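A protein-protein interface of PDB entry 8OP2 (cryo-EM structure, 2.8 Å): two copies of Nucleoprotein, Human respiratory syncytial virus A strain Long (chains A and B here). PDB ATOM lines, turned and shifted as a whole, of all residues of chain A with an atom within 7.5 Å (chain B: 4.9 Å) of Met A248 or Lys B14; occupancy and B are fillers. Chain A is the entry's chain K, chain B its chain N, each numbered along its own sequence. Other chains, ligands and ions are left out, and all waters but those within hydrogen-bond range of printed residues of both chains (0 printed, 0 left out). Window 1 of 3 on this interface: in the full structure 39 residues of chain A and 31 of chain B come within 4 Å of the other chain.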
ATOM      1  N   ALA A 165     -25.086 -11.726 -30.786  1.00  0.00           N
ATOM      2  CA  ALA A 165     -24.626 -10.850 -29.715  1.00  0.00           C
ATOM      3  C   ALA A 165     -25.793 -10.282 -28.924  1.00  0.00           C
ATOM      4  O   ALA A 165     -25.730 -10.183 -27.695  1.00  0.00           O
ATOM      5  CB  ALA A 165     -23.769  -9.725 -30.289  1.00  0.00           C
ATOM      6  N   THR A 169     -26.617 -10.790 -24.977  1.00  0.00           N
ATOM      7  CA  THR A 169     -26.961  -9.741 -24.021  1.00  0.00           C
ATOM      8  C   THR A 169     -28.164 -10.143 -23.184  1.00  0.00           C
ATOM      9  O   THR A 169     -28.203  -9.882 -21.977  1.00  0.00           O
ATOM     10  CB  THR A 169     -27.249  -8.417 -24.731  1.00  0.00           C
ATOM     11  OG1 THR A 169     -28.405  -8.557 -25.566  1.00  0.00           O
ATOM     12  CG2 THR A 169     -26.070  -7.972 -25.566  1.00  0.00           C
ATOM     13  N   GLY A 227     -16.095 -13.309 -29.227  1.00  0.00           N
ATOM     14  CA  GLY A 227     -16.447 -11.903 -29.171  1.00  0.00           C
ATOM     15  C   GLY A 227     -15.370 -11.064 -28.514  1.00  0.00           C
ATOM     16  O   GLY A 227     -15.142  -9.918 -28.902  1.00  0.00           O
ATOM     17  N   ILE A 228     -14.703 -11.618 -27.503  1.00  0.00           N
ATOM     18  CA  ILE A 228     -13.597 -10.897 -26.882  1.00  0.00           C
ATOM     19  C   ILE A 228     -12.424 -10.781 -27.847  1.00  0.00           C
ATOM     20  O   ILE A 228     -11.778  -9.731 -27.934  1.00  0.00           O
ATOM     21  CB  ILE A 228     -13.186 -11.570 -25.563  1.00  0.00           C
ATOM     22  CG1 ILE A 228     -14.332 -11.514 -24.558  1.00  0.00           C
ATOM     23  CG2 ILE A 228     -11.960 -10.896 -24.982  1.00  0.00           C
ATOM     24  CD1 ILE A 228     -14.053 -12.262 -23.286  1.00  0.00           C
ATOM     25  N   SER A 231     -13.321  -8.214 -30.526  1.00  0.00           N
ATOM     26  CA  SER A 231     -13.270  -6.866 -29.981  1.00  0.00           C
ATOM     27  C   SER A 231     -11.855  -6.417 -29.650  1.00  0.00           C
ATOM     28  O   SER A 231     -11.657  -5.242 -29.329  1.00  0.00           O
ATOM     29  CB  SER A 231     -14.149  -6.775 -28.737  1.00  0.00           C
ATOM     30  OG  SER A 231     -15.492  -7.091 -29.046  1.00  0.00           O
ATOM     31  N   ILE A 242     -20.422  -2.676 -35.321  1.00  0.00           N
ATOM     32  CA  ILE A 242     -21.744  -2.901 -34.743  1.00  0.00           C
ATOM     33  C   ILE A 242     -21.724  -4.125 -33.844  1.00  0.00           C
ATOM     34  O   ILE A 242     -22.292  -4.116 -32.746  1.00  0.00           O
ATOM     35  CB  ILE A 242     -22.804  -3.046 -35.851  1.00  0.00           C
ATOM     36  CG1 ILE A 242     -22.925  -1.761 -36.661  1.00  0.00           C
ATOM     37  CG2 ILE A 242     -24.142  -3.397 -35.253  1.00  0.00           C
ATOM     38  CD1 ILE A 242     -23.907  -1.864 -37.791  1.00  0.00           C
ATOM     39  N   PHE A 243     -21.079  -5.202 -34.298  1.00  0.00           N
ATOM     40  CA  PHE A 243     -20.995  -6.407 -33.481  1.00  0.00           C
ATOM     41  C   PHE A 243     -20.254  -6.140 -32.184  1.00  0.00           C
ATOM     42  O   PHE A 243     -20.662  -6.622 -31.127  1.00  0.00           O
ATOM     43  CB  PHE A 243     -20.312  -7.535 -34.250  1.00  0.00           C
ATOM     44  CG  PHE A 243     -19.970  -8.723 -33.395  1.00  0.00           C
ATOM     45  CD1 PHE A 243     -20.908  -9.706 -33.148  1.00  0.00           C
ATOM     46  CD2 PHE A 243     -18.713  -8.856 -32.835  1.00  0.00           C
ATOM     47  CE1 PHE A 243     -20.601 -10.790 -32.362  1.00  0.00           C
ATOM     48  CE2 PHE A 243     -18.405  -9.940 -32.045  1.00  0.00           C
ATOM     49  CZ  PHE A 243     -19.349 -10.907 -31.811  1.00  0.00           C
ATOM     50  N   ALA A 244     -19.154  -5.395 -32.243  1.00  0.00           N
ATOM     51  CA  ALA A 244     -18.406  -5.093 -31.028  1.00  0.00           C
ATOM     52  C   ALA A 244     -19.234  -4.256 -30.064  1.00  0.00           C
ATOM     53  O   ALA A 244     -19.232  -4.501 -28.851  1.00  0.00           O
ATOM     54  CB  ALA A 244     -17.106  -4.381 -31.379  1.00  0.00           C
ATOM     55  N   GLY A 245     -19.959  -3.266 -30.589  1.00  0.00           N
ATOM     56  CA  GLY A 245     -20.805  -2.451 -29.733  1.00  0.00           C
ATOM     57  C   GLY A 245     -21.926  -3.243 -29.090  1.00  0.00           C
ATOM     58  O   GLY A 245     -22.239  -3.047 -27.916  1.00  0.00           O
ATOM     59  N   LEU A 246     -22.547  -4.146 -29.851  1.00  0.00           N
ATOM     60  CA  LEU A 246     -23.618  -4.969 -29.300  1.00  0.00           C
ATOM     61  C   LEU A 246     -23.088  -6.028 -28.344  1.00  0.00           C
ATOM     62  O   LEU A 246     -23.789  -6.421 -27.410  1.00  0.00           O
ATOM     63  CB  LEU A 246     -24.404  -5.638 -30.423  1.00  0.00           C
ATOM     64  CG  LEU A 246     -25.169  -4.725 -31.375  1.00  0.00           C
ATOM     65  CD1 LEU A 246     -25.859  -5.552 -32.435  1.00  0.00           C
ATOM     66  CD2 LEU A 246     -26.167  -3.884 -30.618  1.00  0.00           C
ATOM     67  N   PHE A 247     -21.869  -6.509 -28.568  1.00  0.00           N
ATOM     68  CA  PHE A 247     -21.287  -7.505 -27.684  1.00  0.00           C
ATOM     69  C   PHE A 247     -20.867  -6.905 -26.356  1.00  0.00           C
ATOM     70  O   PHE A 247     -21.055  -7.536 -25.313  1.00  0.00           O
ATOM     71  CB  PHE A 247     -20.089  -8.172 -28.354  1.00  0.00           C
ATOM     72  CG  PHE A 247     -19.480  -9.272 -27.543  1.00  0.00           C
ATOM     73  CD1 PHE A 247     -20.050 -10.528 -27.518  1.00  0.00           C
ATOM     74  CD2 PHE A 247     -18.337  -9.048 -26.800  1.00  0.00           C
ATOM     75  CE1 PHE A 247     -19.491 -11.537 -26.772  1.00  0.00           C
ATOM     76  CE2 PHE A 247     -17.778 -10.051 -26.052  1.00  0.00           C
ATOM     77  CZ  PHE A 247     -18.355 -11.298 -26.037  1.00  0.00           C
ATOM     78  N   MET A 248     -20.300  -5.699 -26.361  1.00  0.00           N
ATOM     79  CA  MET A 248     -19.947  -5.096 -25.086  1.00  0.00           C
ATOM     80  C   MET A 248     -21.166  -4.546 -24.363  1.00  0.00           C
ATOM     81  O   MET A 248     -21.054  -4.136 -23.206  1.00  0.00           O
ATOM     82  CB  MET A 248     -18.897  -4.012 -25.284  1.00  0.00           C
ATOM     83  CG  MET A 248     -17.549  -4.585 -25.667  1.00  0.00           C
ATOM     84  SD  MET A 248     -16.882  -5.699 -24.416  1.00  0.00           S
ATOM     85  CE  MET A 248     -16.185  -4.537 -23.263  1.00  0.00           C
ATOM     86  N   ASN A 249     -22.324  -4.525 -25.021  1.00  0.00           N
ATOM     87  CA  ASN A 249     -23.577  -4.278 -24.322  1.00  0.00           C
ATOM     88  C   ASN A 249     -23.921  -5.409 -23.367  1.00  0.00           C
ATOM     89  O   ASN A 249     -24.738  -5.214 -22.463  1.00  0.00           O
ATOM     90  CB  ASN A 249     -24.716  -4.092 -25.321  1.00  0.00           C
ATOM     91  CG  ASN A 249     -24.769  -2.698 -25.892  1.00  0.00           C
ATOM     92  OD1 ASN A 249     -25.623  -2.387 -26.718  1.00  0.00           O
ATOM     93  ND2 ASN A 249     -23.856  -1.846 -25.451  1.00  0.00           N
ATOM     94  N   ALA A 250     -23.325  -6.584 -23.556  1.00  0.00           N
ATOM     95  CA  ALA A 250     -23.551  -7.724 -22.683  1.00  0.00           C
ATOM     96  C   ALA A 250     -22.647  -7.723 -21.465  1.00  0.00           C
ATOM     97  O   ALA A 250     -22.858  -8.533 -20.559  1.00  0.00           O
ATOM     98  CB  ALA A 250     -23.350  -9.025 -23.459  1.00  0.00           C
ATOM     99  N   TYR A 251     -21.646  -6.849 -21.421  1.00  0.00           N
ATOM    100  CA  TYR A 251     -20.758  -6.786 -20.273  1.00  0.00           C
ATOM    101  C   TYR A 251     -21.532  -6.322 -19.048  1.00  0.00           C
ATOM    102  O   TYR A 251     -22.208  -5.291 -19.082  1.00  0.00           O
ATOM    103  CB  TYR A 251     -19.594  -5.844 -20.565  1.00  0.00           C
ATOM    104  CG  TYR A 251     -18.592  -5.715 -19.445  1.00  0.00           C
ATOM    105  CD1 TYR A 251     -18.788  -4.817 -18.409  1.00  0.00           C
ATOM    106  CD2 TYR A 251     -17.443  -6.483 -19.432  1.00  0.00           C
ATOM    107  CE1 TYR A 251     -17.879  -4.696 -17.395  1.00  0.00           C
ATOM    108  CE2 TYR A 251     -16.526  -6.366 -18.419  1.00  0.00           C
ATOM    109  CZ  TYR A 251     -16.750  -5.471 -17.403  1.00  0.00           C
ATOM    110  OH  TYR A 251     -15.841  -5.349 -16.385  1.00  0.00           O
ATOM    111  N   GLY A 252     -21.427  -7.080 -17.964  1.00  0.00           N
ATOM    112  CA  GLY A 252     -22.157  -6.764 -16.759  1.00  0.00           C
ATOM    113  C   GLY A 252     -23.587  -7.242 -16.732  1.00  0.00           C
ATOM    114  O   GLY A 252     -24.331  -6.860 -15.826  1.00  0.00           O
ATOM    115  N   ALA A 253     -24.001  -8.050 -17.702  1.00  0.00           N
ATOM    116  CA  ALA A 253     -25.345  -8.605 -17.683  1.00  0.00           C
ATOM    117  C   ALA A 253     -25.493  -9.567 -16.518  1.00  0.00           C
ATOM    118  O   ALA A 253     -24.613 -10.390 -16.257  1.00  0.00           O
ATOM    119  CB  ALA A 253     -25.648  -9.318 -18.997  1.00  0.00           C
ATOM    120  N   ARG A 259     -24.343  -1.776 -10.433  1.00  0.00           N
ATOM    121  CA  ARG A 259     -24.394  -0.480 -11.098  1.00  0.00           C
ATOM    122  C   ARG A 259     -25.441   0.422 -10.462  1.00  0.00           C
ATOM    123  O   ARG A 259     -25.209   1.621 -10.275  1.00  0.00           O
ATOM    124  CB  ARG A 259     -24.679  -0.670 -12.585  1.00  0.00           C
ATOM    125  CG  ARG A 259     -23.463  -1.042 -13.413  1.00  0.00           C
ATOM    126  CD  ARG A 259     -23.139  -2.515 -13.288  1.00  0.00           C
ATOM    127  NE  ARG A 259     -21.843  -2.844 -13.865  1.00  0.00           N
ATOM    128  CZ  ARG A 259     -21.259  -4.029 -13.747  1.00  0.00           C
ATOM    129  NH1 ARG A 259     -21.854  -4.994 -13.070  1.00  0.00           N
ATOM    130  NH2 ARG A 259     -20.077  -4.248 -14.301  1.00  0.00           N
ATOM    131  N   GLY A 295     -12.262  -7.581 -11.660  1.00  0.00           N
ATOM    132  CA  GLY A 295     -11.977  -6.729 -12.797  1.00  0.00           C
ATOM    133  C   GLY A 295     -12.749  -7.067 -14.055  1.00  0.00           C
ATOM    134  O   GLY A 295     -13.961  -7.288 -14.009  1.00  0.00           O
ATOM    135  N   GLY A 296     -12.048  -7.103 -15.188  1.00  0.00           N
ATOM    136  CA  GLY A 296     -12.699  -7.267 -16.475  1.00  0.00           C
ATOM    137  C   GLY A 296     -13.356  -8.612 -16.687  1.00  0.00           C
ATOM    138  O   GLY A 296     -14.418  -8.675 -17.314  1.00  0.00           O
ATOM    139  N   GLU A 297     -12.749  -9.688 -16.188  1.00  0.00           N
ATOM    140  CA  GLU A 297     -13.286 -11.020 -16.439  1.00  0.00           C
ATOM    141  C   GLU A 297     -14.659 -11.212 -15.809  1.00  0.00           C
ATOM    142  O   GLU A 297     -15.431 -12.058 -16.267  1.00  0.00           O
ATOM    143  CB  GLU A 297     -12.317 -12.080 -15.919  1.00  0.00           C
ATOM    144  CG  GLU A 297     -12.080 -12.012 -14.424  1.00  0.00           C
ATOM    145  CD  GLU A 297     -11.192 -13.132 -13.920  1.00  0.00           C
ATOM    146  OE1 GLU A 297     -11.659 -14.289 -13.885  1.00  0.00           O
ATOM    147  OE2 GLU A 297     -10.032 -12.853 -13.555  1.00  0.00           O
ATOM    148  N   PHE A 300     -18.673 -11.136 -17.593  1.00  0.00           N
ATOM    149  CA  PHE A 300     -19.359 -12.204 -18.309  1.00  0.00           C
ATOM    150  C   PHE A 300     -19.590 -13.430 -17.436  1.00  0.00           C
ATOM    151  O   PHE A 300     -19.786 -14.528 -17.959  1.00  0.00           O
ATOM    152  CB  PHE A 300     -18.579 -12.589 -19.568  1.00  0.00           C
ATOM    153  CG  PHE A 300     -18.625 -11.549 -20.647  1.00  0.00           C
ATOM    154  CD1 PHE A 300     -19.699 -11.476 -21.509  1.00  0.00           C
ATOM    155  CD2 PHE A 300     -17.598 -10.640 -20.793  1.00  0.00           C
ATOM    156  CE1 PHE A 300     -19.746 -10.522 -22.493  1.00  0.00           C
ATOM    157  CE2 PHE A 300     -17.645  -9.684 -21.775  1.00  0.00           C
ATOM    158  CZ  PHE A 300     -18.717  -9.625 -22.624  1.00  0.00           C
ATOM    159  N   ASP B  10     -15.908   0.636 -14.672  1.00  0.00           N
ATOM    160  CA  ASP B  10     -16.347  -0.197 -15.787  1.00  0.00           C
ATOM    161  C   ASP B  10     -15.512   0.039 -17.040  1.00  0.00           C
ATOM    162  O   ASP B  10     -15.184  -0.912 -17.755  1.00  0.00           O
ATOM    163  CB  ASP B  10     -17.826   0.047 -16.076  1.00  0.00           C
ATOM    164  CG  ASP B  10     -18.731  -0.817 -15.229  1.00  0.00           C
ATOM    165  OD1 ASP B  10     -18.215  -1.736 -14.562  1.00  0.00           O
ATOM    166  OD2 ASP B  10     -19.957  -0.583 -15.231  1.00  0.00           O
ATOM    167  N   THR B  11     -15.170   1.294 -17.331  1.00  0.00           N
ATOM    168  CA  THR B  11     -14.391   1.594 -18.530  1.00  0.00           C
ATOM    169  C   THR B  11     -13.033   0.905 -18.491  1.00  0.00           C
ATOM    170  O   THR B  11     -12.614   0.259 -19.460  1.00  0.00           O
ATOM    171  CB  THR B  11     -14.216   3.108 -18.669  1.00  0.00           C
ATOM    172  OG1 THR B  11     -15.497   3.748 -18.640  1.00  0.00           O
ATOM    173  CG2 THR B  11     -13.512   3.455 -19.967  1.00  0.00           C
ATOM    174  N   LEU B  12     -12.336   1.024 -17.363  1.00  0.00           N
ATOM    175  CA  LEU B  12     -11.010   0.433 -17.233  1.00  0.00           C
ATOM    176  C   LEU B  12     -11.080  -1.087 -17.242  1.00  0.00           C
ATOM    177  O   LEU B  12     -10.206  -1.752 -17.806  1.00  0.00           O
ATOM    178  CB  LEU B  12     -10.351   0.942 -15.955  1.00  0.00           C
ATOM    179  CG  LEU B  12      -8.917   0.522 -15.658  1.00  0.00           C
ATOM    180  CD1 LEU B  12      -7.944   1.386 -16.440  1.00  0.00           C
ATOM    181  CD2 LEU B  12      -8.646   0.611 -14.170  1.00  0.00           C
ATOM    182  N   ASN B  13     -12.115  -1.656 -16.623  1.00  0.00           N
ATOM    183  CA  ASN B  13     -12.269  -3.105 -16.614  1.00  0.00           C
ATOM    184  C   ASN B  13     -12.563  -3.642 -18.008  1.00  0.00           C
ATOM    185  O   ASN B  13     -12.030  -4.687 -18.401  1.00  0.00           O
ATOM    186  CB  ASN B  13     -13.371  -3.502 -15.637  1.00  0.00           C
ATOM    187  CG  ASN B  13     -12.973  -3.293 -14.195  1.00  0.00           C
ATOM    188  OD1 ASN B  13     -11.795  -3.140 -13.882  1.00  0.00           O
ATOM    189  ND2 ASN B  13     -13.955  -3.280 -13.307  1.00  0.00           N
ATOM    190  N   LYS B  14     -13.405  -2.945 -18.772  1.00  0.00           N
ATOM    191  CA  LYS B  14     -13.650  -3.335 -20.156  1.00  0.00           C
ATOM    192  C   LYS B  14     -12.379  -3.248 -20.986  1.00  0.00           C
ATOM    193  O   LYS B  14     -12.102  -4.135 -21.803  1.00  0.00           O
ATOM    194  CB  LYS B  14     -14.732  -2.453 -20.771  1.00  0.00           C
ATOM    195  CG  LYS B  14     -16.102  -2.615 -20.170  1.00  0.00           C
ATOM    196  CD  LYS B  14     -17.127  -1.857 -20.979  1.00  0.00           C
ATOM    197  CE  LYS B  14     -18.472  -1.851 -20.290  1.00  0.00           C
ATOM    198  NZ  LYS B  14     -19.535  -1.301 -21.162  1.00  0.00           N
ATOM    199  N   ASP B  15     -11.596  -2.185 -20.798  1.00  0.00           N
ATOM    200  CA  ASP B  15     -10.336  -2.080 -21.523  1.00  0.00           C
ATOM    201  C   ASP B  15      -9.392  -3.216 -21.168  1.00  0.00           C
ATOM    202  O   ASP B  15      -8.727  -3.771 -22.046  1.00  0.00           O
ATOM    203  CB  ASP B  15      -9.670  -0.734 -21.256  1.00  0.00           C
ATOM    204  CG  ASP B  15      -8.317  -0.617 -21.930  1.00  0.00           C
ATOM    205  OD1 ASP B  15      -7.317  -1.073 -21.338  1.00  0.00           O
ATOM    206  OD2 ASP B  15      -8.248  -0.114 -23.068  1.00  0.00           O
ATOM    207  N   GLN B  16      -9.300  -3.565 -19.886  1.00  0.00           N
ATOM    208  CA  GLN B  16      -8.413  -4.657 -19.502  1.00  0.00           C
ATOM    209  C   GLN B  16      -8.898  -5.982 -20.071  1.00  0.00           C
ATOM    210  O   GLN B  16      -8.090  -6.820 -20.482  1.00  0.00           O
ATOM    211  CB  GLN B  16      -8.281  -4.727 -17.982  1.00  0.00           C
ATOM    212  CG  GLN B  16      -7.519  -5.942 -17.490  1.00  0.00           C
ATOM    213  CD  GLN B  16      -8.244  -6.679 -16.389  1.00  0.00           C
ATOM    214  OE1 GLN B  16      -9.159  -6.142 -15.768  1.00  0.00           O
ATOM    215  NE2 GLN B  16      -7.840  -7.917 -16.142  1.00  0.00           N
ATOM    216  N   LEU B  17     -10.214  -6.187 -20.117  1.00  0.00           N
ATOM    217  CA  LEU B  17     -10.740  -7.406 -20.720  1.00  0.00           C
ATOM    218  C   LEU B  17     -10.394  -7.483 -22.201  1.00  0.00           C
ATOM    219  O   LEU B  17     -10.022  -8.548 -22.705  1.00  0.00           O
ATOM    220  CB  LEU B  17     -12.251  -7.487 -20.526  1.00  0.00           C
ATOM    221  CG  LEU B  17     -12.911  -8.718 -21.144  1.00  0.00           C
ATOM    222  CD1 LEU B  17     -12.572  -9.958 -20.346  1.00  0.00           C
ATOM    223  CD2 LEU B  17     -14.407  -8.535 -21.217  1.00  0.00           C
ATOM    224  N   LEU B  18     -10.518  -6.367 -22.918  1.00  0.00           N
ATOM    225  CA  LEU B  18     -10.246  -6.388 -24.351  1.00  0.00           C
ATOM    226  C   LEU B  18      -8.758  -6.458 -24.663  1.00  0.00           C
ATOM    227  O   LEU B  18      -8.374  -7.016 -25.695  1.00  0.00           O
ATOM    228  CB  LEU B  18     -10.869  -5.165 -25.019  1.00  0.00           C
ATOM    229  CG  LEU B  18     -12.394  -5.167 -24.958  1.00  0.00           C
ATOM    230  CD1 LEU B  18     -12.976  -4.052 -25.801  1.00  0.00           C
ATOM    231  CD2 LEU B  18     -12.932  -6.514 -25.393  1.00  0.00           C
ATOM    232  N   LEU B 311     -15.747   2.849 -25.982  1.00  0.00           N
ATOM    233  CA  LEU B 311     -15.382   3.135 -24.602  1.00  0.00           C
ATOM    234  C   LEU B 311     -15.037   4.598 -24.377  1.00  0.00           C
ATOM    235  O   LEU B 311     -15.017   5.044 -23.228  1.00  0.00           O
ATOM    236  CB  LEU B 311     -14.203   2.264 -24.173  1.00  0.00           C
ATOM    237  CG  LEU B 311     -14.362   0.752 -24.308  1.00  0.00           C
ATOM    238  CD1 LEU B 311     -13.187   0.045 -23.670  1.00  0.00           C
ATOM    239  CD2 LEU B 311     -15.657   0.297 -23.683  1.00  0.00           C
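The side-chain carboxylate of Asp B10 lies within salt-bridge range of the guanidinium group of Arg A259, at 3.1 Å. The backbone NH (N) of Gly A296 sits at hydrogen-bond distance from the side-chain amide oxygen (OE1) of Gln B16 (3.1 Å).
O of Gly A227 sits at hydrogen-bond distance from OG of Ser A231, 2.9 Å away.
Among the printed residues, pairs that only touch across the chains: Ile A228 with Leu B17 (3.8 Å), Ser A231 with Leu B18 (3.6 Å), Met A248 with Lys B14 (3.6 Å), Tyr A251 with Asn B13 (3.2 Å), Tyr A251 with Lys B14 (3.5 Å), Gly A295 with Asn B13 (3.8 Å), Gly A296 with Asn B13 (3.3 Å), Gly A296 with Leu B17 (3.8 Å) and Phe A300 with Leu B17 (3.5 Å).
Met A248 touches just one residue of chain B: Lys B14. Lys B14 touches just these residues of chain A: Met A248 (3.6 Å) and Tyr A251 (3.5 Å). Of the printed residues of chain B, Gly A295 touches Asn B13 (3.8 Å). Printed residues of chain B within 4 Å of Tyr A251: Asn B13 and Lys B14. Of the printed residues of chain B, Ser A231 touches Leu B18. Of the printed residues of chain A, Asn B13 touches Tyr A251 (3.2 Å), Gly A295 (3.8 Å) and Gly A296 (3.3 Å). Of the printed residues of chain B, Gly A296 touches Asn B13, Gln B16 and Leu B17. The nearest residue of chain B that does not touch Met A248 is Leu B18 (4.1 Å). The nearest residue of chain A that does not touch Lys B14 is Gly A296 (4.9 Å). The nearest printed residue of chain A that does not touch Asp B10 is Tyr A251 (4.1 Å).
Printed residues of chain A that touch a printed residue of chain B: Ile A228, Ser A231, Met A248, Tyr A251, Arg A259, Gly A295, Gly A296 and Phe A300. Hydrophobic or aromatic side chains of chain A that line the printed part of chain B: Ile A228, Met A248, Tyr A251 and Phe A300. Along chain A the printed residues that touch a printed residue of chain B span positions 228 to 300. Printed residues of chain B that touch a printed residue of chain A: Asp B10, Asn B13, Lys B14, Gln B16, Leu B17 and Leu B18.
No position is printed for both chains.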
